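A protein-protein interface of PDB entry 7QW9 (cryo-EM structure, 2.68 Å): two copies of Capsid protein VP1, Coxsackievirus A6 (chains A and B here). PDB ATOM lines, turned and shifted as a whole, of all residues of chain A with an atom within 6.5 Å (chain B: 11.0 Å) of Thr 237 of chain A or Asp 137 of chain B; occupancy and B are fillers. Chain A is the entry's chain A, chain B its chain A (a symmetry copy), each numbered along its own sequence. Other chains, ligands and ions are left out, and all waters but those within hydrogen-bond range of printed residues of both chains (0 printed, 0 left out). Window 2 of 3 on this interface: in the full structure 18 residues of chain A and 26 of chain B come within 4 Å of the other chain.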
ATOM      1  N   ASP A  92      15.931 -14.994  -6.779  1.00  0.00           N
ATOM      2  CA  ASP A  92      16.139 -16.355  -6.220  1.00  0.00           C
ATOM      3  C   ASP A  92      15.688 -16.439  -4.757  1.00  0.00           C
ATOM      4  O   ASP A  92      16.250 -17.272  -4.025  1.00  0.00           O
ATOM      5  CB  ASP A  92      17.603 -16.761  -6.356  1.00  0.00           C
ATOM      6  CG  ASP A  92      17.815 -18.261  -6.459  1.00  0.00           C
ATOM      7  OD1 ASP A  92      16.801 -19.018  -6.383  1.00  0.00           O
ATOM      8  OD2 ASP A  92      18.998 -18.664  -6.640  1.00  0.00           O
ATOM      9  N   SER A  93      14.691 -15.656  -4.341  1.00  0.00           N
ATOM     10  CA  SER A  93      14.228 -15.612  -2.928  1.00  0.00           C
ATOM     11  C   SER A  93      12.724 -15.361  -2.859  1.00  0.00           C
ATOM     12  O   SER A  93      12.164 -14.822  -3.841  1.00  0.00           O
ATOM     13  CB  SER A  93      14.991 -14.573  -2.138  1.00  0.00           C
ATOM     14  OG  SER A  93      14.734 -13.263  -2.630  1.00  0.00           O
ATOM     15  N   GLY A  99      16.004 -18.317  -9.824  1.00  0.00           N
ATOM     16  CA  GLY A  99      17.471 -18.212  -9.911  1.00  0.00           C
ATOM     17  C   GLY A  99      17.955 -18.028 -11.338  1.00  0.00           C
ATOM     18  O   GLY A  99      19.146 -18.260 -11.577  1.00  0.00           O
ATOM     19  N   GLY A 142      31.860 -13.321  -4.265  1.00  0.00           N
ATOM     20  CA  GLY A 142      32.414 -14.258  -5.258  1.00  0.00           C
ATOM     21  C   GLY A 142      31.331 -15.153  -5.824  1.00  0.00           C
ATOM     22  O   GLY A 142      31.452 -16.368  -5.687  1.00  0.00           O
ATOM     23  N   MET A 143      30.307 -14.590  -6.456  1.00  0.00           N
ATOM     24  CA  MET A 143      29.101 -15.350  -6.850  1.00  0.00           C
ATOM     25  C   MET A 143      29.097 -15.481  -8.368  1.00  0.00           C
ATOM     26  O   MET A 143      29.063 -14.461  -9.041  1.00  0.00           O
ATOM     27  CB  MET A 143      27.869 -14.599  -6.375  1.00  0.00           C
ATOM     28  CG  MET A 143      26.630 -15.403  -6.433  1.00  0.00           C
ATOM     29  SD  MET A 143      25.466 -14.709  -5.267  1.00  0.00           S
ATOM     30  CE  MET A 143      23.918 -15.126  -6.069  1.00  0.00           C
ATOM     31  N   LEU A 144      29.169 -16.694  -8.892  1.00  0.00           N
ATOM     32  CA  LEU A 144      29.333 -16.941 -10.348  1.00  0.00           C
ATOM     33  C   LEU A 144      28.003 -16.775 -11.073  1.00  0.00           C
ATOM     34  O   LEU A 144      26.981 -17.251 -10.534  1.00  0.00           O
ATOM     35  CB  LEU A 144      29.851 -18.358 -10.533  1.00  0.00           C
ATOM     36  CG  LEU A 144      30.318 -18.679 -11.934  1.00  0.00           C
ATOM     37  CD1 LEU A 144      31.496 -17.811 -12.343  1.00  0.00           C
ATOM     38  CD2 LEU A 144      30.684 -20.131 -11.992  1.00  0.00           C
ATOM     39  N   ARG A 160      16.722 -23.270 -13.901  1.00  0.00           N
ATOM     40  CA  ARG A 160      18.081 -22.899 -13.439  1.00  0.00           C
ATOM     41  C   ARG A 160      19.094 -23.841 -14.077  1.00  0.00           C
ATOM     42  O   ARG A 160      20.056 -23.350 -14.681  1.00  0.00           O
ATOM     43  CB  ARG A 160      18.138 -22.999 -11.921  1.00  0.00           C
ATOM     44  CG  ARG A 160      19.515 -22.755 -11.326  1.00  0.00           C
ATOM     45  CD  ARG A 160      19.537 -23.304  -9.914  1.00  0.00           C
ATOM     46  NE  ARG A 160      18.329 -22.947  -9.178  1.00  0.00           N
ATOM     47  CZ  ARG A 160      18.186 -21.903  -8.383  1.00  0.00           C
ATOM     48  NH1 ARG A 160      19.176 -21.048  -8.179  1.00  0.00           N
ATOM     49  NH2 ARG A 160      17.033 -21.721  -7.770  1.00  0.00           N
ATOM     50  N   THR A 231      22.397 -17.533 -11.843  1.00  0.00           N
ATOM     51  CA  THR A 231      23.475 -17.852 -10.880  1.00  0.00           C
ATOM     52  C   THR A 231      23.778 -19.336 -11.076  1.00  0.00           C
ATOM     53  O   THR A 231      22.845 -20.141 -10.979  1.00  0.00           O
ATOM     54  CB  THR A 231      23.066 -17.474  -9.455  1.00  0.00           C
ATOM     55  OG1 THR A 231      21.919 -18.227  -9.062  1.00  0.00           O
ATOM     56  CG2 THR A 231      22.729 -16.007  -9.330  1.00  0.00           C
ATOM     57  N   VAL A 232      25.010 -19.681 -11.413  1.00  0.00           N
ATOM     58  CA  VAL A 232      25.406 -21.075 -11.712  1.00  0.00           C
ATOM     59  C   VAL A 232      25.363 -21.822 -10.386  1.00  0.00           C
ATOM     60  O   VAL A 232      26.410 -21.918  -9.764  1.00  0.00           O
ATOM     61  CB  VAL A 232      26.800 -21.132 -12.361  1.00  0.00           C
ATOM     62  CG1 VAL A 232      27.092 -22.524 -12.880  1.00  0.00           C
ATOM     63  CG2 VAL A 232      26.974 -20.136 -13.497  1.00  0.00           C
ATOM     64  N   SER A 233      24.199 -22.298  -9.948  1.00  0.00           N
ATOM     65  CA  SER A 233      24.003 -22.963  -8.630  1.00  0.00           C
ATOM     66  C   SER A 233      23.158 -24.242  -8.750  1.00  0.00           C
ATOM     67  O   SER A 233      22.636 -24.522  -9.835  1.00  0.00           O
ATOM     68  CB  SER A 233      23.391 -21.996  -7.671  1.00  0.00           C
ATOM     69  OG  SER A 233      22.120 -21.576  -8.126  1.00  0.00           O
ATOM     70  N   GLU A 234      23.033 -24.993  -7.662  1.00  0.00           N
ATOM     71  CA  GLU A 234      22.267 -26.263  -7.611  1.00  0.00           C
ATOM     72  C   GLU A 234      20.885 -26.028  -7.020  1.00  0.00           C
ATOM     73  O   GLU A 234      20.012 -26.861  -7.235  1.00  0.00           O
ATOM     74  CB  GLU A 234      23.007 -27.291  -6.762  1.00  0.00           C
ATOM     75  CG  GLU A 234      24.412 -27.544  -7.259  1.00  0.00           C
ATOM     76  CD  GLU A 234      24.462 -27.911  -8.731  1.00  0.00           C
ATOM     77  OE1 GLU A 234      23.916 -28.994  -9.076  1.00  0.00           O
ATOM     78  OE2 GLU A 234      25.021 -27.101  -9.535  1.00  0.00           O
ATOM     79  N   SER A 235      20.712 -24.961  -6.255  1.00  0.00           N
ATOM     80  CA  SER A 235      19.516 -24.745  -5.413  1.00  0.00           C
ATOM     81  C   SER A 235      19.361 -23.251  -5.195  1.00  0.00           C
ATOM     82  O   SER A 235      20.271 -22.502  -5.615  1.00  0.00           O
ATOM     83  CB  SER A 235      19.633 -25.475  -4.100  1.00  0.00           C
ATOM     84  OG  SER A 235      19.612 -26.882  -4.288  1.00  0.00           O
ATOM     85  N   THR A 236      18.261 -22.847  -4.571  1.00  0.00           N
ATOM     86  CA  THR A 236      17.955 -21.425  -4.301  1.00  0.00           C
ATOM     87  C   THR A 236      19.082 -20.828  -3.438  1.00  0.00           C
ATOM     88  O   THR A 236      19.407 -21.419  -2.394  1.00  0.00           O
ATOM     89  CB  THR A 236      16.541 -21.290  -3.727  1.00  0.00           C
ATOM     90  OG1 THR A 236      16.257 -19.888  -3.707  1.00  0.00           O
ATOM     91  CG2 THR A 236      16.371 -21.901  -2.351  1.00  0.00           C
ATOM     92  N   THR A 237      19.684 -19.720  -3.877  1.00  0.00           N
ATOM     93  CA  THR A 237      20.772 -19.015  -3.165  1.00  0.00           C
ATOM     94  C   THR A 237      20.146 -18.125  -2.098  1.00  0.00           C
ATOM     95  O   THR A 237      20.896 -17.625  -1.256  1.00  0.00           O
ATOM     96  CB  THR A 237      21.642 -18.188  -4.123  1.00  0.00           C
ATOM     97  OG1 THR A 237      20.871 -17.131  -4.705  1.00  0.00           O
ATOM     98  CG2 THR A 237      22.255 -19.023  -5.229  1.00  0.00           C
ATOM     99  N   GLY A 238      18.839 -17.873  -2.185  1.00  0.00           N
ATOM    100  CA  GLY A 238      18.116 -16.934  -1.306  1.00  0.00           C
ATOM    101  C   GLY A 238      18.559 -15.484  -1.478  1.00  0.00           C
ATOM    102  O   GLY A 238      18.249 -14.686  -0.573  1.00  0.00           O
ATOM    103  N   LYS A 239      19.220 -15.130  -2.590  1.00  0.00           N
ATOM    104  CA  LYS A 239      19.715 -13.753  -2.868  1.00  0.00           C
ATOM    105  C   LYS A 239      19.282 -13.322  -4.270  1.00  0.00           C
ATOM    106  O   LYS A 239      19.504 -14.106  -5.214  1.00  0.00           O
ATOM    107  CB  LYS A 239      21.238 -13.705  -2.728  1.00  0.00           C
ATOM    108  CG  LYS A 239      21.740 -13.906  -1.304  1.00  0.00           C
ATOM    109  CD  LYS A 239      23.224 -13.656  -1.119  1.00  0.00           C
ATOM    110  CE  LYS A 239      24.101 -14.555  -1.967  1.00  0.00           C
ATOM    111  NZ  LYS A 239      23.890 -15.994  -1.670  1.00  0.00           N
ATOM    112  N   ASN A 240      18.711 -12.120  -4.401  1.00  0.00           N
ATOM    113  CA  ASN A 240      18.349 -11.503  -5.702  1.00  0.00           C
ATOM    114  C   ASN A 240      19.566 -10.742  -6.216  1.00  0.00           C
ATOM    115  O   ASN A 240      20.224 -10.091  -5.400  1.00  0.00           O
ATOM    116  CB  ASN A 240      17.146 -10.570  -5.582  1.00  0.00           C
ATOM    117  CG  ASN A 240      15.991 -11.208  -4.845  1.00  0.00           C
ATOM    118  OD1 ASN A 240      15.246 -12.003  -5.408  1.00  0.00           O
ATOM    119  ND2 ASN A 240      15.845 -10.877  -3.573  1.00  0.00           N
ATOM    120  N   VAL A 241      19.829 -10.800  -7.522  1.00  0.00           N
ATOM    121  CA  VAL A 241      20.967 -10.116  -8.203  1.00  0.00           C
ATOM    122  C   VAL A 241      20.397  -9.125  -9.211  1.00  0.00           C
ATOM    123  O   VAL A 241      19.558  -9.538 -10.035  1.00  0.00           O
ATOM    124  CB  VAL A 241      21.870 -11.137  -8.905  1.00  0.00           C
ATOM    125  CG1 VAL A 241      23.112 -10.488  -9.478  1.00  0.00           C
ATOM    126  CG2 VAL A 241      22.257 -12.269  -7.972  1.00  0.00           C
ATOM    127  N   GLU B  89      31.692 -33.622 -10.121  1.00  0.00           N
ATOM    128  CA  GLU B  89      31.345 -33.231  -8.742  1.00  0.00           C
ATOM    129  C   GLU B  89      32.420 -33.767  -7.794  1.00  0.00           C
ATOM    130  O   GLU B  89      32.478 -34.977  -7.633  1.00  0.00           O
ATOM    131  CB  GLU B  89      29.956 -33.749  -8.413  1.00  0.00           C
ATOM    132  CG  GLU B  89      29.414 -33.079  -7.170  1.00  0.00           C
ATOM    133  CD  GLU B  89      27.924 -33.232  -6.912  1.00  0.00           C
ATOM    134  OE1 GLU B  89      27.152 -33.348  -7.906  1.00  0.00           O
ATOM    135  OE2 GLU B  89      27.542 -33.232  -5.699  1.00  0.00           O
ATOM    136  N   SER B 133      34.577 -23.595 -12.008  1.00  0.00           N
ATOM    137  CA  SER B 133      34.397 -24.319 -10.729  1.00  0.00           C
ATOM    138  C   SER B 133      33.743 -23.409  -9.703  1.00  0.00           C
ATOM    139  O   SER B 133      34.119 -22.259  -9.670  1.00  0.00           O
ATOM    140  CB  SER B 133      35.709 -24.802 -10.249  1.00  0.00           C
ATOM    141  OG  SER B 133      36.168 -25.855 -11.079  1.00  0.00           O
ATOM    142  N   ASN B 134      32.851 -23.916  -8.864  1.00  0.00           N
ATOM    143  CA  ASN B 134      32.119 -23.119  -7.843  1.00  0.00           C
ATOM    144  C   ASN B 134      31.526 -24.076  -6.813  1.00  0.00           C
ATOM    145  O   ASN B 134      31.746 -25.284  -6.962  1.00  0.00           O
ATOM    146  CB  ASN B 134      31.034 -22.251  -8.475  1.00  0.00           C
ATOM    147  CG  ASN B 134      30.052 -23.048  -9.309  1.00  0.00           C
ATOM    148  OD1 ASN B 134      30.399 -23.571 -10.372  1.00  0.00           O
ATOM    149  ND2 ASN B 134      28.816 -23.144  -8.848  1.00  0.00           N
ATOM    150  N   LEU B 135      30.807 -23.562  -5.811  1.00  0.00           N
ATOM    151  CA  LEU B 135      30.165 -24.374  -4.746  1.00  0.00           C
ATOM    152  C   LEU B 135      28.676 -24.553  -5.062  1.00  0.00           C
ATOM    153  O   LEU B 135      28.271 -24.188  -6.166  1.00  0.00           O
ATOM    154  CB  LEU B 135      30.388 -23.680  -3.402  1.00  0.00           C
ATOM    155  CG  LEU B 135      31.820 -23.695  -2.866  1.00  0.00           C
ATOM    156  CD1 LEU B 135      31.830 -23.277  -1.401  1.00  0.00           C
ATOM    157  CD2 LEU B 135      32.473 -25.061  -3.008  1.00  0.00           C
ATOM    158  N   ASN B 136      27.904 -25.164  -4.159  1.00  0.00           N
ATOM    159  CA  ASN B 136      26.443 -25.386  -4.319  1.00  0.00           C
ATOM    160  C   ASN B 136      25.708 -24.040  -4.350  1.00  0.00           C
ATOM    161  O   ASN B 136      24.710 -23.953  -5.077  1.00  0.00           O
ATOM    162  CB  ASN B 136      25.875 -26.302  -3.234  1.00  0.00           C
ATOM    163  CG  ASN B 136      26.137 -27.769  -3.524  1.00  0.00           C
ATOM    164  OD1 ASN B 136      27.204 -28.301  -3.207  1.00  0.00           O
ATOM    165  ND2 ASN B 136      25.175 -28.438  -4.138  1.00  0.00           N
ATOM    166  N   ASP B 137      26.192 -23.025  -3.625  1.00  0.00           N
ATOM    167  CA  ASP B 137      25.563 -21.679  -3.539  1.00  0.00           C
ATOM    168  C   ASP B 137      26.143 -20.741  -4.597  1.00  0.00           C
ATOM    169  O   ASP B 137      26.079 -19.527  -4.401  1.00  0.00           O
ATOM    170  CB  ASP B 137      25.759 -21.082  -2.143  1.00  0.00           C
ATOM    171  CG  ASP B 137      24.961 -21.777  -1.049  1.00  0.00           C
ATOM    172  OD1 ASP B 137      24.065 -22.605  -1.392  1.00  0.00           O
ATOM    173  OD2 ASP B 137      25.225 -21.478   0.147  1.00  0.00           O
ATOM    174  N   SER B 138      26.704 -21.271  -5.678  1.00  0.00           N
ATOM    175  CA  SER B 138      27.400 -20.513  -6.749  1.00  0.00           C
ATOM    176  C   SER B 138      28.501 -19.598  -6.201  1.00  0.00           C
ATOM    177  O   SER B 138      28.854 -18.671  -6.922  1.00  0.00           O
ATOM    178  CB  SER B 138      26.422 -19.724  -7.584  1.00  0.00           C
ATOM    179  OG  SER B 138      25.924 -18.596  -6.892  1.00  0.00           O
ATOM    180  N   THR B 139      29.054 -19.849  -5.013  1.00  0.00           N
ATOM    181  CA  THR B 139      30.100 -18.995  -4.384  1.00  0.00           C
ATOM    182  C   THR B 139      31.475 -19.540  -4.769  1.00  0.00           C
ATOM    183  O   THR B 139      31.600 -20.753  -4.900  1.00  0.00           O
ATOM    184  CB  THR B 139      29.926 -18.936  -2.868  1.00  0.00           C
ATOM    185  OG1 THR B 139      29.813 -20.282  -2.396  1.00  0.00           O
ATOM    186  CG2 THR B 139      28.720 -18.122  -2.457  1.00  0.00           C
ATOM    187  N   THR B 140      32.472 -18.677  -4.933  1.00  0.00           N
ATOM    188  CA  THR B 140      33.866 -19.053  -5.286  1.00  0.00           C
ATOM    189  C   THR B 140      34.807 -18.539  -4.193  1.00  0.00           C
ATOM    190  O   THR B 140      35.432 -17.491  -4.369  1.00  0.00           O
ATOM    191  CB  THR B 140      34.228 -18.530  -6.681  1.00  0.00           C
ATOM    192  OG1 THR B 140      33.921 -17.140  -6.739  1.00  0.00           O
ATOM    193  CG2 THR B 140      33.505 -19.225  -7.814  1.00  0.00           C
ATOM    194  N   PRO B 141      34.975 -19.250  -3.045  1.00  0.00           N
ATOM    195  CA  PRO B 141      35.938 -18.852  -2.018  1.00  0.00           C
ATOM    196  C   PRO B 141      37.391 -19.117  -2.449  1.00  0.00           C
ATOM    197  O   PRO B 141      37.628 -19.659  -3.526  1.00  0.00           O
ATOM    198  CB  PRO B 141      35.601 -19.727  -0.807  1.00  0.00           C
ATOM    199  CG  PRO B 141      34.304 -20.385  -1.173  1.00  0.00           C
ATOM    200  CD  PRO B 141      34.319 -20.503  -2.680  1.00  0.00           C
ATOM    201  N   LEU B 177      39.249 -21.493  -6.559  1.00  0.00           N
ATOM    202  CA  LEU B 177      37.888 -21.211  -7.072  1.00  0.00           C
ATOM    203  C   LEU B 177      37.752 -19.704  -7.292  1.00  0.00           C
ATOM    204  O   LEU B 177      37.100 -19.326  -8.276  1.00  0.00           O
ATOM    205  CB  LEU B 177      36.829 -21.681  -6.088  1.00  0.00           C
ATOM    206  CG  LEU B 177      36.822 -23.163  -5.760  1.00  0.00           C
ATOM    207  CD1 LEU B 177      35.700 -23.450  -4.789  1.00  0.00           C
ATOM    208  CD2 LEU B 177      36.668 -24.014  -6.995  1.00  0.00           C
ATOM    209  N   GLY B 238      34.108 -30.772   4.050  1.00  0.00           N
ATOM    210  CA  GLY B 238      32.644 -30.752   4.229  1.00  0.00           C
ATOM    211  C   GLY B 238      31.917 -29.939   3.162  1.00  0.00           C
ATOM    212  O   GLY B 238      30.744 -29.599   3.409  1.00  0.00           O
ATOM    213  N   LYS B 239      32.548 -29.660   2.012  1.00  0.00           N
ATOM    214  CA  LYS B 239      31.951 -28.866   0.901  1.00  0.00           C
ATOM    215  C   LYS B 239      32.131 -29.614  -0.422  1.00  0.00           C
ATOM    216  O   LYS B 239      33.269 -30.039  -0.700  1.00  0.00           O
ATOM    217  CB  LYS B 239      32.601 -27.482   0.838  1.00  0.00           C
ATOM    218  CG  LYS B 239      32.281 -26.589   2.030  1.00  0.00           C
ATOM    219  CD  LYS B 239      32.745 -25.153   1.881  1.00  0.00           C
ATOM    220  CE  LYS B 239      34.242 -25.016   1.687  1.00  0.00           C
ATOM    221  NZ  LYS B 239      35.013 -25.578   2.824  1.00  0.00           N
ATOM    222  N   ASN B 240      31.058 -29.747  -1.210  1.00  0.00           N
ATOM    223  CA  ASN B 240      31.090 -30.332  -2.573  1.00  0.00           C
ATOM    224  C   ASN B 240      31.407 -29.213  -3.559  1.00  0.00           C
ATOM    225  O   ASN B 240      30.862 -28.120  -3.381  1.00  0.00           O
ATOM    226  CB  ASN B 240      29.771 -31.010  -2.940  1.00  0.00           C
ATOM    227  CG  ASN B 240      29.286 -31.951  -1.862  1.00  0.00           C
ATOM    228  OD1 ASN B 240      29.765 -33.074  -1.745  1.00  0.00           O
ATOM    229  ND2 ASN B 240      28.343 -31.493  -1.056  1.00  0.00           N
ATOM    230  N   VAL B 241      32.230 -29.489  -4.571  1.00  0.00           N
ATOM    231  CA  VAL B 241      32.646 -28.525  -5.631  1.00  0.00           C
ATOM    232  C   VAL B 241      32.163 -29.055  -6.976  1.00  0.00           C
ATOM    233  O   VAL B 241      32.452 -30.226  -7.288  1.00  0.00           O
ATOM    234  CB  VAL B 241      34.169 -28.354  -5.637  1.00  0.00           C
ATOM    235  CG1 VAL B 241      34.609 -27.272  -6.602  1.00  0.00           C
ATOM    236  CG2 VAL B 241      34.701 -28.058  -4.248  1.00  0.00           C
ATOM    237  N   HIS B 242      31.463 -28.235  -7.762  1.00  0.00           N
ATOM    238  CA  HIS B 242      31.023 -28.592  -9.133  1.00  0.00           C
ATOM    239  C   HIS B 242      32.025 -28.023 -10.118  1.00  0.00           C
ATOM    240  O   HIS B 242      32.303 -26.838 -10.025  1.00  0.00           O
ATOM    241  CB  HIS B 242      29.631 -28.066  -9.432  1.00  0.00           C
ATOM    242  CG  HIS B 242      28.680 -28.455  -8.373  1.00  0.00           C
ATOM    243  ND1 HIS B 242      28.063 -29.686  -8.375  1.00  0.00           N
ATOM    244  CD2 HIS B 242      28.303 -27.813  -7.243  1.00  0.00           C
ATOM    245  CE1 HIS B 242      27.299 -29.782  -7.303  1.00  0.00           C
ATOM    246  NE2 HIS B 242      27.434 -28.641  -6.581  1.00  0.00           N
ATOM    247  N   ARG B 244      32.319 -27.568 -14.019  1.00  0.00           N
ATOM    248  CA  ARG B 244      31.812 -27.553 -15.395  1.00  0.00           C
ATOM    249  C   ARG B 244      33.015 -27.435 -16.324  1.00  0.00           C
ATOM    250  O   ARG B 244      33.681 -26.390 -16.295  1.00  0.00           O
ATOM    251  CB  ARG B 244      30.831 -26.403 -15.558  1.00  0.00           C
ATOM    252  CG  ARG B 244      29.517 -26.693 -14.871  1.00  0.00           C
ATOM    253  CD  ARG B 244      28.558 -25.539 -14.952  1.00  0.00           C
ATOM    254  NE  ARG B 244      27.367 -25.817 -14.161  1.00  0.00           N
ATOM    255  CZ  ARG B 244      27.312 -25.792 -12.834  1.00  0.00           C
ATOM    256  NH1 ARG B 244      28.383 -25.481 -12.114  1.00  0.00           N
ATOM    257  NH2 ARG B 244      26.165 -26.062 -12.232  1.00  0.00           N
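O of Gly 142 of chain A lies within hydrogen-bond range of N of Thr 140 of chain B, at 2.6 Å. The backbone NH of Leu 144 of chain A is in hydrogen-bond range of the backbone carbonyl oxygen of Ser 138 of chain B. ND2 of Asn 134 of chain B is in hydrogen-bond range of O of Val 232 of chain A. The backbone carbonyl oxygen (O) of Asn 136 of chain B sits at hydrogen-bond distance from the backbone NH (N) of Glu 234 of chain A (3.3 Å). OE2 of Glu 234 of chain A lies within salt-bridge range of NH2 of Arg 244 of chain B (3.1 Å).
O of Gly 99 of chain A is in hydrogen-bond range of N of Thr 231 of chain A, at 3.3 Å. The backbone carbonyl oxygen of Leu 144 of chain A lies within hydrogen-bond range of the backbone NH of Val 232 of chain A, 3.2 Å away. OG of Ser 233 of chain A sits at hydrogen-bond distance from NH1 of Arg 160 of chain A (3.0 Å). The side-chain hydroxyl (OG) of Ser 233 of chain A sits at hydrogen-bond distance from the backbone carbonyl oxygen (O) of Thr 231 of chain A. OG1 of Thr 237 of chain A lies close to N of Lys 239 of chain A, 3.3 Å away. A ring nitrogen (NE2) of His 242 of chain B lies within hydrogen-bond range of the side-chain amide nitrogen (ND2) of Asn 136 of chain B, 3.3 Å away.
Among the printed residues, merely in contact across the chains: Gly 142 of chain A with Ser 138 of chain B, Gly 142 of chain A with Thr 139 of chain B, Met 143 of chain A with Ser 138 of chain B, Leu 144 of chain A with Asn 134 of chain B, Thr 231 of chain A with Ser 138 of chain B, Val 232 of chain A with Ser 138 of chain B, Val 232 of chain A with Arg 244 of chain B, Ser 233 of chain A with Asn 136 of chain B, Ser 233 of chain A with Ser 138 of chain B, Glu 234 of chain A with His 242 of chain B and Thr 237 of chain A with Asp 137 of chain B.
No residue of chain B comes within 4 Å of Asp 92 of chain A. Ser 93 of chain A touches none of the printed residues of chain B. Printed residues of chain B within 4 Å of Leu 144 of chain A: Asn 134 and Ser 138. Printed residues of chain B within 4 Å of Thr 231 of chain A: Ser 138 (3.9995 Å). No residue of chain B comes within 4 Å of Ser 235 of chain A. No residue of chain B comes within 4 Å of Thr 236 of chain A. Thr 237 of chain A touches one residue of chain B. No residue of chain B comes within 4 Å of Gly 238 of chain A. No residue of chain B comes within 4 Å of Lys 239 of chain A. Of chain A, only Thr 237 (3.9 Å) comes within 4 Å of Asp 137 of chain B. The nearest residue of chain B that does not touch Thr 237 of chain A is Ser 138 of chain B (4.1 Å). The nearest printed residue of chain A that does not touch Asn 134 of chain B is Ser 233 of chain A (4.8 Å).
Hydrophobic or aromatic side chains of chain A within 4 Å of the printed part of chain B: Met 143, Leu 144 and Val 232. Hydrophobic or aromatic side chains of chain B within 4 Å of the printed part of chain A: His 242. Among the printed residues, 16 pairs touch across the chains. Among the printed residues, Asp or Glu carboxylates within 4 Å of a Lys or Arg side-chain nitrogen of the other chain: Glu 234 of chain A with Arg 244 of chain B.
Positions printed for both chains: 238, 239, 240 and 241. Of the 16 pairs that touch across the chains among the printed residues, none has its exchanged pair printed and touching as well.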
